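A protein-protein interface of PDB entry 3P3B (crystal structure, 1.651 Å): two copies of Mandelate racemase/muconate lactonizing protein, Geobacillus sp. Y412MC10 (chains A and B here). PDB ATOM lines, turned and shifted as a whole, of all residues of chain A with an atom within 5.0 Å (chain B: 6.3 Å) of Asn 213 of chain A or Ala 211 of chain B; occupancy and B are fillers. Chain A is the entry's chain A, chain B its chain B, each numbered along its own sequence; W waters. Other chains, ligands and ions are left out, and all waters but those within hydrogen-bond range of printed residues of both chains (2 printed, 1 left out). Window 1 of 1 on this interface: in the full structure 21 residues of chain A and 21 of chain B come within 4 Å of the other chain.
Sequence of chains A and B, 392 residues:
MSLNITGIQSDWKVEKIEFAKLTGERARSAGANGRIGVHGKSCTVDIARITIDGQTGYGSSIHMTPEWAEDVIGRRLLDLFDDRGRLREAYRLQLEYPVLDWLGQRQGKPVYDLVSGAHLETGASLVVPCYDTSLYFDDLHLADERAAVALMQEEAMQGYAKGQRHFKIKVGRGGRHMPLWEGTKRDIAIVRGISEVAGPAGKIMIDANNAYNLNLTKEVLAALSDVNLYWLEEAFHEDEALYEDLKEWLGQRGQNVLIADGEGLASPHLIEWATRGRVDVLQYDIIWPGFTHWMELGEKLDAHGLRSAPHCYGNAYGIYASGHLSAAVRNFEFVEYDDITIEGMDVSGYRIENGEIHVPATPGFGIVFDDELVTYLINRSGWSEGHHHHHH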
ATOM      1  N   ALA A 211     -23.174 -33.431  -0.331  1.00  0.00           N
ATOM      2  CA  ALA A 211     -23.973 -34.331  -1.172  1.00  0.00           C
ATOM      3  C   ALA A 211     -25.462 -33.983  -1.193  1.00  0.00           C
ATOM      4  O   ALA A 211     -26.198 -34.546  -1.991  1.00  0.00           O
ATOM      5  CB  ALA A 211     -23.791 -35.788  -0.747  1.00  0.00           C
ATOM      6  N   TYR A 212     -25.896 -33.069  -0.333  1.00  0.00           N
ATOM      7  CA  TYR A 212     -27.327 -32.696  -0.318  1.00  0.00           C
ATOM      8  C   TYR A 212     -27.589 -31.445  -1.151  1.00  0.00           C
ATOM      9  O   TYR A 212     -26.665 -30.803  -1.643  1.00  0.00           O
ATOM     10  CB  TYR A 212     -27.826 -32.469   1.113  1.00  0.00           C
ATOM     11  CG  TYR A 212     -28.001 -33.698   2.010  1.00  0.00           C
ATOM     12  CD1 TYR A 212     -28.062 -35.000   1.498  1.00  0.00           C
ATOM     13  CD2 TYR A 212     -28.093 -33.538   3.380  1.00  0.00           C
ATOM     14  CE1 TYR A 212     -28.249 -36.107   2.355  1.00  0.00           C
ATOM     15  CE2 TYR A 212     -28.243 -34.612   4.222  1.00  0.00           C
ATOM     16  CZ  TYR A 212     -28.331 -35.885   3.721  1.00  0.00           C
ATOM     17  OH  TYR A 212     -28.498 -36.911   4.627  1.00  0.00           O
ATOM     18  N   ASN A 213     -28.863 -31.103  -1.334  1.00  0.00           N
ATOM     19  CA  ASN A 213     -29.222 -29.727  -1.674  1.00  0.00           C
ATOM     20  C   ASN A 213     -30.130 -29.208  -0.566  1.00  0.00           C
ATOM     21  O   ASN A 213     -30.375 -29.926   0.400  1.00  0.00           O
ATOM     22  CB  ASN A 213     -29.861 -29.620  -3.061  1.00  0.00           C
ATOM     23  CG  ASN A 213     -31.106 -30.481  -3.208  1.00  0.00           C
ATOM     24  OD1 ASN A 213     -31.713 -30.893  -2.223  1.00  0.00           O
ATOM     25  ND2 ASN A 213     -31.485 -30.758  -4.443  1.00  0.00           N
ATOM     26  N   LEU A 214     -30.638 -27.980  -0.686  1.00  0.00           N
ATOM     27  CA  LEU A 214     -31.368 -27.392   0.430  1.00  0.00           C
ATOM     28  C   LEU A 214     -32.598 -28.234   0.830  1.00  0.00           C
ATOM     29  O   LEU A 214     -32.814 -28.510   2.012  1.00  0.00           O
ATOM     30  CB  LEU A 214     -31.752 -25.944   0.129  1.00  0.00           C
ATOM     31  CG  LEU A 214     -32.509 -25.218   1.249  1.00  0.00           C
ATOM     32  CD1 LEU A 214     -31.733 -25.298   2.557  1.00  0.00           C
ATOM     33  CD2 LEU A 214     -32.860 -23.753   0.879  1.00  0.00           C
ATOM     34  N   ASN A 215     -33.402 -28.631  -0.149  1.00  0.00           N
ATOM     35  CA  ASN A 215     -34.604 -29.423   0.138  1.00  0.00           C
ATOM     36  C   ASN A 215     -34.328 -30.828   0.676  1.00  0.00           C
ATOM     37  O   ASN A 215     -35.025 -31.293   1.572  1.00  0.00           O
ATOM     38  CB  ASN A 215     -35.577 -29.445  -1.048  1.00  0.00           C
ATOM     39  CG  ASN A 215     -36.500 -28.213  -1.064  1.00  0.00           C
ATOM     40  OD1 ASN A 215     -36.774 -27.619  -0.019  1.00  0.00           O
ATOM     41  ND2 ASN A 215     -36.948 -27.809  -2.249  1.00  0.00           N
ATOM     42  N   LEU A 216     -33.300 -31.500   0.163  1.00  0.00           N
ATOM     43  CA  LEU A 216     -32.903 -32.765   0.772  1.00  0.00           C
ATOM     44  C   LEU A 216     -32.526 -32.548   2.225  1.00  0.00           C
ATOM     45  O   LEU A 216     -32.872 -33.353   3.085  1.00  0.00           O
ATOM     46  CB  LEU A 216     -31.731 -33.392   0.034  1.00  0.00           C
ATOM     47  CG  LEU A 216     -32.054 -34.357  -1.091  1.00  0.00           C
ATOM     48  CD1 LEU A 216     -30.798 -34.636  -1.910  1.00  0.00           C
ATOM     49  CD2 LEU A 216     -32.672 -35.635  -0.540  1.00  0.00           C
ATOM     50  N   THR A 217     -31.809 -31.458   2.491  1.00  0.00           N
ATOM     51  CA  THR A 217     -31.383 -31.141   3.860  1.00  0.00           C
ATOM     52  C   THR A 217     -32.584 -30.940   4.784  1.00  0.00           C
ATOM     53  O   THR A 217     -32.646 -31.483   5.902  1.00  0.00           O
ATOM     54  CB  THR A 217     -30.448 -29.914   3.895  1.00  0.00           C
ATOM     55  OG1 THR A 217     -29.322 -30.126   3.021  1.00  0.00           O
ATOM     56  CG2 THR A 217     -29.963 -29.635   5.323  1.00  0.00           C
ATOM     57  N   ALA A 235     -23.709 -29.461   4.410  1.00  0.00           N
ATOM     58  CA  ALA A 235     -24.907 -30.050   3.809  1.00  0.00           C
ATOM     59  C   ALA A 235     -24.779 -29.933   2.295  1.00  0.00           C
ATOM     60  O   ALA A 235     -25.123 -30.843   1.554  1.00  0.00           O
ATOM     61  CB  ALA A 235     -26.173 -29.317   4.312  1.00  0.00           C
ATOM     62  N   PHE A 236     -24.261 -28.791   1.862  1.00  0.00           N
ATOM     63  CA  PHE A 236     -23.980 -28.494   0.461  1.00  0.00           C
ATOM     64  C   PHE A 236     -22.906 -27.426   0.483  1.00  0.00           C
ATOM     65  O   PHE A 236     -22.645 -26.835   1.522  1.00  0.00           O
ATOM     66  CB  PHE A 236     -25.220 -27.923  -0.226  1.00  0.00           C
ATOM     67  CG  PHE A 236     -26.039 -27.036   0.664  1.00  0.00           C
ATOM     68  CD1 PHE A 236     -27.197 -27.519   1.268  1.00  0.00           C
ATOM     69  CD2 PHE A 236     -25.656 -25.730   0.907  1.00  0.00           C
ATOM     70  CE1 PHE A 236     -27.964 -26.715   2.095  1.00  0.00           C
ATOM     71  CE2 PHE A 236     -26.433 -24.907   1.750  1.00  0.00           C
ATOM     72  CZ  PHE A 236     -27.575 -25.408   2.336  1.00  0.00           C
ATOM     73  N   GLY B  34     -32.314 -21.835  -9.501  1.00  0.00           N
ATOM     74  CA  GLY B  34     -32.229 -22.913  -8.538  1.00  0.00           C
ATOM     75  C   GLY B  34     -31.927 -22.499  -7.103  1.00  0.00           C
ATOM     76  O   GLY B  34     -32.309 -23.208  -6.182  1.00  0.00           O
ATOM     77  N   ARG B  35     -31.236 -21.375  -6.917  1.00  0.00           N
ATOM     78  CA  ARG B  35     -30.694 -21.003  -5.608  1.00  0.00           C
ATOM     79  C   ARG B  35     -31.263 -19.721  -5.013  1.00  0.00           C
ATOM     80  O   ARG B  35     -31.255 -19.558  -3.794  1.00  0.00           O
ATOM     81  CB  ARG B  35     -29.156 -20.902  -5.647  1.00  0.00           C
ATOM     82  CG  ARG B  35     -28.606 -19.913  -6.673  1.00  0.00           C
ATOM     83  CD  ARG B  35     -27.082 -19.742  -6.510  1.00  0.00           C
ATOM     84  NE  ARG B  35     -26.776 -19.128  -5.222  1.00  0.00           N
ATOM     85  CZ  ARG B  35     -26.665 -17.817  -5.012  1.00  0.00           C
ATOM     86  NH1 ARG B  35     -26.394 -17.370  -3.795  1.00  0.00           N
ATOM     87  NH2 ARG B  35     -26.795 -16.943  -6.013  1.00  0.00           N
ATOM     88  N   VAL B 171     -32.782 -25.007 -14.527  1.00  0.00           N
ATOM     89  CA  VAL B 171     -33.349 -26.173 -13.849  1.00  0.00           C
ATOM     90  C   VAL B 171     -32.944 -26.166 -12.369  1.00  0.00           C
ATOM     91  O   VAL B 171     -32.326 -25.219 -11.920  1.00  0.00           O
ATOM     92  CB  VAL B 171     -32.999 -27.501 -14.550  1.00  0.00           C
ATOM     93  CG1 VAL B 171     -33.574 -27.501 -15.974  1.00  0.00           C
ATOM     94  CG2 VAL B 171     -31.463 -27.782 -14.556  1.00  0.00           C
ATOM     95  N   GLY B 172     -33.300 -27.216 -11.632  1.00  0.00           N
ATOM     96  CA  GLY B 172     -33.112 -27.242 -10.187  1.00  0.00           C
ATOM     97  C   GLY B 172     -34.294 -26.685  -9.385  1.00  0.00           C
ATOM     98  O   GLY B 172     -34.134 -26.204  -8.252  1.00  0.00           O
ATOM     99  N   ARG B 173     -35.490 -26.757  -9.958  1.00  0.00           N
ATOM    100  CA  ARG B 173     -36.667 -26.279  -9.241  1.00  0.00           C
ATOM    101  C   ARG B 173     -36.809 -26.926  -7.860  1.00  0.00           C
ATOM    102  O   ARG B 173     -37.273 -26.283  -6.920  1.00  0.00           O
ATOM    103  CB  ARG B 173     -37.932 -26.519 -10.074  1.00  0.00           C
ATOM    104  CG  ARG B 173     -38.050 -25.550 -11.238  1.00  0.00           C
ATOM    105  CD  ARG B 173     -39.100 -26.004 -12.252  1.00  0.00           C
ATOM    106  NE  ARG B 173     -39.293 -24.962 -13.250  1.00  0.00           N
ATOM    107  CZ  ARG B 173     -38.440 -24.703 -14.229  1.00  0.00           C
ATOM    108  NH1 ARG B 173     -38.684 -23.704 -15.072  1.00  0.00           N
ATOM    109  NH2 ARG B 173     -37.332 -25.435 -14.360  1.00  0.00           N
ATOM    110  N   GLY B 174     -36.409 -28.194  -7.762  1.00  0.00           N
ATOM    111  CA  GLY B 174     -36.551 -28.981  -6.552  1.00  0.00           C
ATOM    112  C   GLY B 174     -35.508 -28.716  -5.476  1.00  0.00           C
ATOM    113  O   GLY B 174     -35.628 -29.222  -4.356  1.00  0.00           O
ATOM    114  N   GLY B 175     -34.500 -27.915  -5.803  1.00  0.00           N
ATOM    115  CA  GLY B 175     -33.444 -27.581  -4.863  1.00  0.00           C
ATOM    116  C   GLY B 175     -33.901 -26.757  -3.680  1.00  0.00           C
ATOM    117  O   GLY B 175     -33.514 -27.013  -2.539  1.00  0.00           O
ATOM    118  N   ARG B 176     -34.736 -25.761  -3.957  1.00  0.00           N
ATOM    119  CA  ARG B 176     -35.180 -24.832  -2.934  1.00  0.00           C
ATOM    120  C   ARG B 176     -36.647 -24.423  -3.104  1.00  0.00           C
ATOM    121  O   ARG B 176     -37.379 -24.283  -2.120  1.00  0.00           O
ATOM    122  CB  ARG B 176     -34.325 -23.575  -3.001  1.00  0.00           C
ATOM    123  CG  ARG B 176     -34.792 -22.489  -2.072  1.00  0.00           C
ATOM    124  CD  ARG B 176     -33.829 -21.346  -2.037  1.00  0.00           C
ATOM    125  NE  ARG B 176     -34.238 -20.399  -1.018  1.00  0.00           N
ATOM    126  CZ  ARG B 176     -33.795 -19.148  -0.918  1.00  0.00           C
ATOM    127  NH1 ARG B 176     -32.914 -18.666  -1.778  1.00  0.00           N
ATOM    128  NH2 ARG B 176     -34.246 -18.381   0.055  1.00  0.00           N
ATOM    129  N   LEU B 180     -38.725 -31.496  -3.785  1.00  0.00           N
ATOM    130  CA  LEU B 180     -37.607 -32.073  -4.518  1.00  0.00           C
ATOM    131  C   LEU B 180     -38.036 -32.856  -5.748  1.00  0.00           C
ATOM    132  O   LEU B 180     -37.656 -32.520  -6.865  1.00  0.00           O
ATOM    133  CB  LEU B 180     -36.802 -32.972  -3.593  1.00  0.00           C
ATOM    134  CG  LEU B 180     -35.543 -33.563  -4.227  1.00  0.00           C
ATOM    135  CD1 LEU B 180     -34.648 -32.452  -4.747  1.00  0.00           C
ATOM    136  CD2 LEU B 180     -34.838 -34.416  -3.196  1.00  0.00           C
ATOM    137  N   ALA B 208     -28.348 -25.645 -13.569  1.00  0.00           N
ATOM    138  CA  ALA B 208     -29.015 -25.928 -12.299  1.00  0.00           C
ATOM    139  C   ALA B 208     -28.674 -24.947 -11.171  1.00  0.00           C
ATOM    140  O   ALA B 208     -29.190 -25.085 -10.058  1.00  0.00           O
ATOM    141  CB  ALA B 208     -28.741 -27.366 -11.864  1.00  0.00           C
ATOM    142  N   ASN B 209     -27.821 -23.967 -11.447  1.00  0.00           N
ATOM    143  CA  ASN B 209     -27.263 -23.120 -10.395  1.00  0.00           C
ATOM    144  C   ASN B 209     -26.948 -23.875  -9.103  1.00  0.00           C
ATOM    145  O   ASN B 209     -27.334 -23.455  -7.988  1.00  0.00           O
ATOM    146  CB  ASN B 209     -28.153 -21.894 -10.133  1.00  0.00           C
ATOM    147  CG  ASN B 209     -28.190 -20.953 -11.318  1.00  0.00           C
ATOM    148  OD1 ASN B 209     -29.044 -21.076 -12.189  1.00  0.00           O
ATOM    149  ND2 ASN B 209     -27.252 -20.008 -11.358  1.00  0.00           N
ATOM    150  N   ASN B 210     -26.248 -24.995  -9.270  1.00  0.00           N
ATOM    151  CA  ASN B 210     -25.764 -25.826  -8.165  1.00  0.00           C
ATOM    152  C   ASN B 210     -26.837 -26.561  -7.367  1.00  0.00           C
ATOM    153  O   ASN B 210     -26.544 -27.166  -6.346  1.00  0.00           O
ATOM    154  CB  ASN B 210     -24.851 -24.992  -7.251  1.00  0.00           C
ATOM    155  CG  ASN B 210     -23.517 -24.668  -7.922  1.00  0.00           C
ATOM    156  OD1 ASN B 210     -23.141 -25.322  -8.892  1.00  0.00           O
ATOM    157  ND2 ASN B 210     -22.818 -23.650  -7.428  1.00  0.00           N
ATOM    158  N   ALA B 211     -28.081 -26.543  -7.842  1.00  0.00           N
ATOM    159  CA  ALA B 211     -29.168 -27.127  -7.050  1.00  0.00           C
ATOM    160  C   ALA B 211     -29.290 -28.657  -7.064  1.00  0.00           C
ATOM    161  O   ALA B 211     -30.112 -29.205  -6.339  1.00  0.00           O
ATOM    162  CB  ALA B 211     -30.513 -26.460  -7.385  1.00  0.00           C
ATOM    163  N   TYR B 212     -28.485 -29.360  -7.860  1.00  0.00           N
ATOM    164  CA  TYR B 212     -28.542 -30.819  -7.859  1.00  0.00           C
ATOM    165  C   TYR B 212     -27.410 -31.418  -7.027  1.00  0.00           C
ATOM    166  O   TYR B 212     -26.528 -30.714  -6.551  1.00  0.00           O
ATOM    167  CB  TYR B 212     -28.430 -31.406  -9.270  1.00  0.00           C
ATOM    168  CG  TYR B 212     -29.572 -31.138 -10.227  1.00  0.00           C
ATOM    169  CD1 TYR B 212     -30.856 -30.852  -9.771  1.00  0.00           C
ATOM    170  CD2 TYR B 212     -29.369 -31.213 -11.606  1.00  0.00           C
ATOM    171  CE1 TYR B 212     -31.904 -30.611 -10.678  1.00  0.00           C
ATOM    172  CE2 TYR B 212     -30.408 -30.989 -12.516  1.00  0.00           C
ATOM    173  CZ  TYR B 212     -31.672 -30.696 -12.045  1.00  0.00           C
ATOM    174  OH  TYR B 212     -32.695 -30.476 -12.947  1.00  0.00           O
ATOM    175  N   ASN B 213     -27.463 -32.726  -6.845  1.00  0.00           N
ATOM    176  CA  ASN B 213     -26.280 -33.503  -6.503  1.00  0.00           C
ATOM    177  C   ASN B 213     -26.016 -34.470  -7.657  1.00  0.00           C
ATOM    178  O   ASN B 213     -26.730 -34.446  -8.672  1.00  0.00           O
ATOM    179  CB  ASN B 213     -26.437 -34.231  -5.161  1.00  0.00           C
ATOM    180  CG  ASN B 213     -27.636 -35.162  -5.127  1.00  0.00           C
ATOM    181  OD1 ASN B 213     -28.156 -35.568  -6.168  1.00  0.00           O
ATOM    182  ND2 ASN B 213     -28.069 -35.526  -3.918  1.00  0.00           N
ATOM    183  N   LEU B 216     -29.118 -36.889  -8.626  1.00  0.00           N
ATOM    184  CA  LEU B 216     -30.180 -36.101  -9.245  1.00  0.00           C
ATOM    185  C   LEU B 216     -29.793 -35.739 -10.674  1.00  0.00           C
ATOM    186  O   LEU B 216     -30.599 -35.852 -11.592  1.00  0.00           O
ATOM    187  CB  LEU B 216     -30.450 -34.819  -8.465  1.00  0.00           C
ATOM    188  CG  LEU B 216     -31.521 -34.858  -7.391  1.00  0.00           C
ATOM    189  CD1 LEU B 216     -31.659 -33.476  -6.731  1.00  0.00           C
ATOM    190  CD2 LEU B 216     -32.845 -35.311  -8.006  1.00  0.00           C
ATOM    191  N   GLU B 234     -23.200 -25.905 -14.147  1.00  0.00           N
ATOM    192  CA  GLU B 234     -23.323 -25.849 -12.695  1.00  0.00           C
ATOM    193  C   GLU B 234     -24.412 -26.777 -12.145  1.00  0.00           C
ATOM    194  O   GLU B 234     -25.354 -26.330 -11.496  1.00  0.00           O
ATOM    195  CB  GLU B 234     -23.514 -24.401 -12.240  1.00  0.00           C
ATOM    196  CG  GLU B 234     -22.249 -23.550 -12.422  1.00  0.00           C
ATOM    197  CD  GLU B 234     -22.189 -22.353 -11.480  1.00  0.00           C
ATOM    198  OE1 GLU B 234     -23.166 -21.578 -11.402  1.00  0.00           O
ATOM    199  OE2 GLU B 234     -21.151 -22.168 -10.813  1.00  0.00           O
ATOM    200  N   ALA B 235     -24.275 -28.072 -12.415  1.00  0.00           N
ATOM    201  CA  ALA B 235     -25.161 -29.065 -11.819  1.00  0.00           C
ATOM    202  C   ALA B 235     -25.062 -29.035 -10.280  1.00  0.00           C
ATOM    203  O   ALA B 235     -26.065 -29.168  -9.563  1.00  0.00           O
ATOM    204  CB  ALA B 235     -24.815 -30.443 -12.336  1.00  0.00           C
ATOM    205  N   PHE B 236     -23.837 -28.872  -9.787  1.00  0.00           N
ATOM    206  CA  PHE B 236     -23.546 -28.843  -8.357  1.00  0.00           C
ATOM    207  C   PHE B 236     -22.197 -28.164  -8.269  1.00  0.00           C
ATOM    208  O   PHE B 236     -21.474 -28.112  -9.269  1.00  0.00           O
ATOM    209  CB  PHE B 236     -23.457 -30.259  -7.771  1.00  0.00           C
ATOM    210  CG  PHE B 236     -22.804 -31.264  -8.698  1.00  0.00           C
ATOM    211  CD1 PHE B 236     -23.565 -32.181  -9.395  1.00  0.00           C
ATOM    212  CD2 PHE B 236     -21.429 -31.267  -8.892  1.00  0.00           C
ATOM    213  CE1 PHE B 236     -22.970 -33.088 -10.259  1.00  0.00           C
ATOM    214  CE2 PHE B 236     -20.832 -32.177  -9.752  1.00  0.00           C
ATOM    215  CZ  PHE B 236     -21.596 -33.083 -10.428  1.00  0.00           C
HETATM  216  O   HOH W   1     -24.833 -31.263  -4.016  1.00  0.00           O
HETATM  217  O   HOH W   2     -36.199 -25.024   0.473  1.00  0.00           O
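The guanidinium group (NH1) of Arg 176 of chain B lies within hydrogen-bond range of the backbone carbonyl oxygen (O) of Arg 35 of chain B, at 2.8 Å. O of Asn 213 of chain A sits at hydrogen-bond distance from OG1 of Thr 217 of chain A (2.8 Å). The side-chain amide oxygen (OD1) of Asn 213 of chain A sits at hydrogen-bond distance from the backbone NH (N) of Leu 216 of chain A (2.9 Å). OD1 of Asn 213 of chain B lies within hydrogen-bond range of N of Leu 216 of chain B (3.0 Å).
Hydrophobic or aromatic side chains of chain B within 4 Å of the printed part of chain A: Leu 180 and Leu 216. Hydrophobic or aromatic side chains of chain A within 4 Å of the printed part of chain B: Leu 214 and Leu 216. Among the printed residues, 12 pairs touch across the chains. Among the printed residues, no Asp or Glu carboxylate lies within 4 Å of a Lys or Arg side-chain nitrogen of the other chain.
Water W2 lies within hydrogen-bond range of the side-chain amide oxygen of Asn 215 of chain A and the backbone carbonyl oxygen of Arg 176 of chain B. Water W1 bridges O of Tyr 212 of chain A (3.0 Å) and O of Tyr 212 of chain B (3.1 Å).
The backbone carbonyl oxygen of Ala 211 of chain A is in hydrogen-bond range of the side-chain amide nitrogen of Asn 213 of chain B (2.9 Å). The backbone carbonyl oxygen of Ala 211 of chain B sits at hydrogen-bond distance from the side-chain amide nitrogen of Asn 213 of chain A (2.8 Å). N of Asn 215 of chain A is in hydrogen-bond range of O of Gly 175 of chain B (2.9 Å). The side-chain amide nitrogen (ND2) of Asn 215 of chain A lies close to the backbone NH (N) of Arg 176 of chain B (3.5 Å). The side-chain amide nitrogen of Asn 215 of chain A lies within hydrogen-bond range of the backbone carbonyl oxygen of Gly 174 of chain B, 2.9 Å away.
Asn 213 of chain A touches just these residues of chain B: Gly 175 (3.8 Å), Leu 180 (3.6 Å), Ala 211 (2.8 Å) and Leu 216 (3.6 Å). Printed residues of chain B within 4 Å of Leu 214 of chain A: Gly 175 (3.4 Å) and Arg 176 (3.7 Å). Printed residues of chain A within 4 Å of Arg 176 of chain B: Leu 214 and Asn 215. Printed residues of chain A within 4 Å of Ala 211 of chain B: Asn 213.
Gly 175 of chain B touches Asn 213 of chain A. Leu 180 of chain B touches Asn 213 of chain A (CD1 to ND2, 3.6 Å). Asn 213 of chain A touches Leu 216 of chain B (ND2 to CD1, 3.6 Å). Leu 214 of chain A touches Gly 175 of chain B. Arg 176 of chain B touches Leu 214 of chain A. Leu 216 of chain A touches Leu 180 of chain B (CG to CD2, 3.5 Å). Leu 216 of chain A touches Asn 213 of chain B (CD1 to ND2, 3.5 Å).
Ala 211 of chain A touches Asn 213 of chain B, and with the chains exchanged Asn 213 of chain A touches Ala 211 of chain B. Asn 213 of chain A touches Leu 216 of chain B, and with the chains exchanged Leu 216 of chain A touches Asn 213 of chain B. Of the 12 pairs that touch across the chains among the printed residues, 4 have their exchanged pair printed and touching as well.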
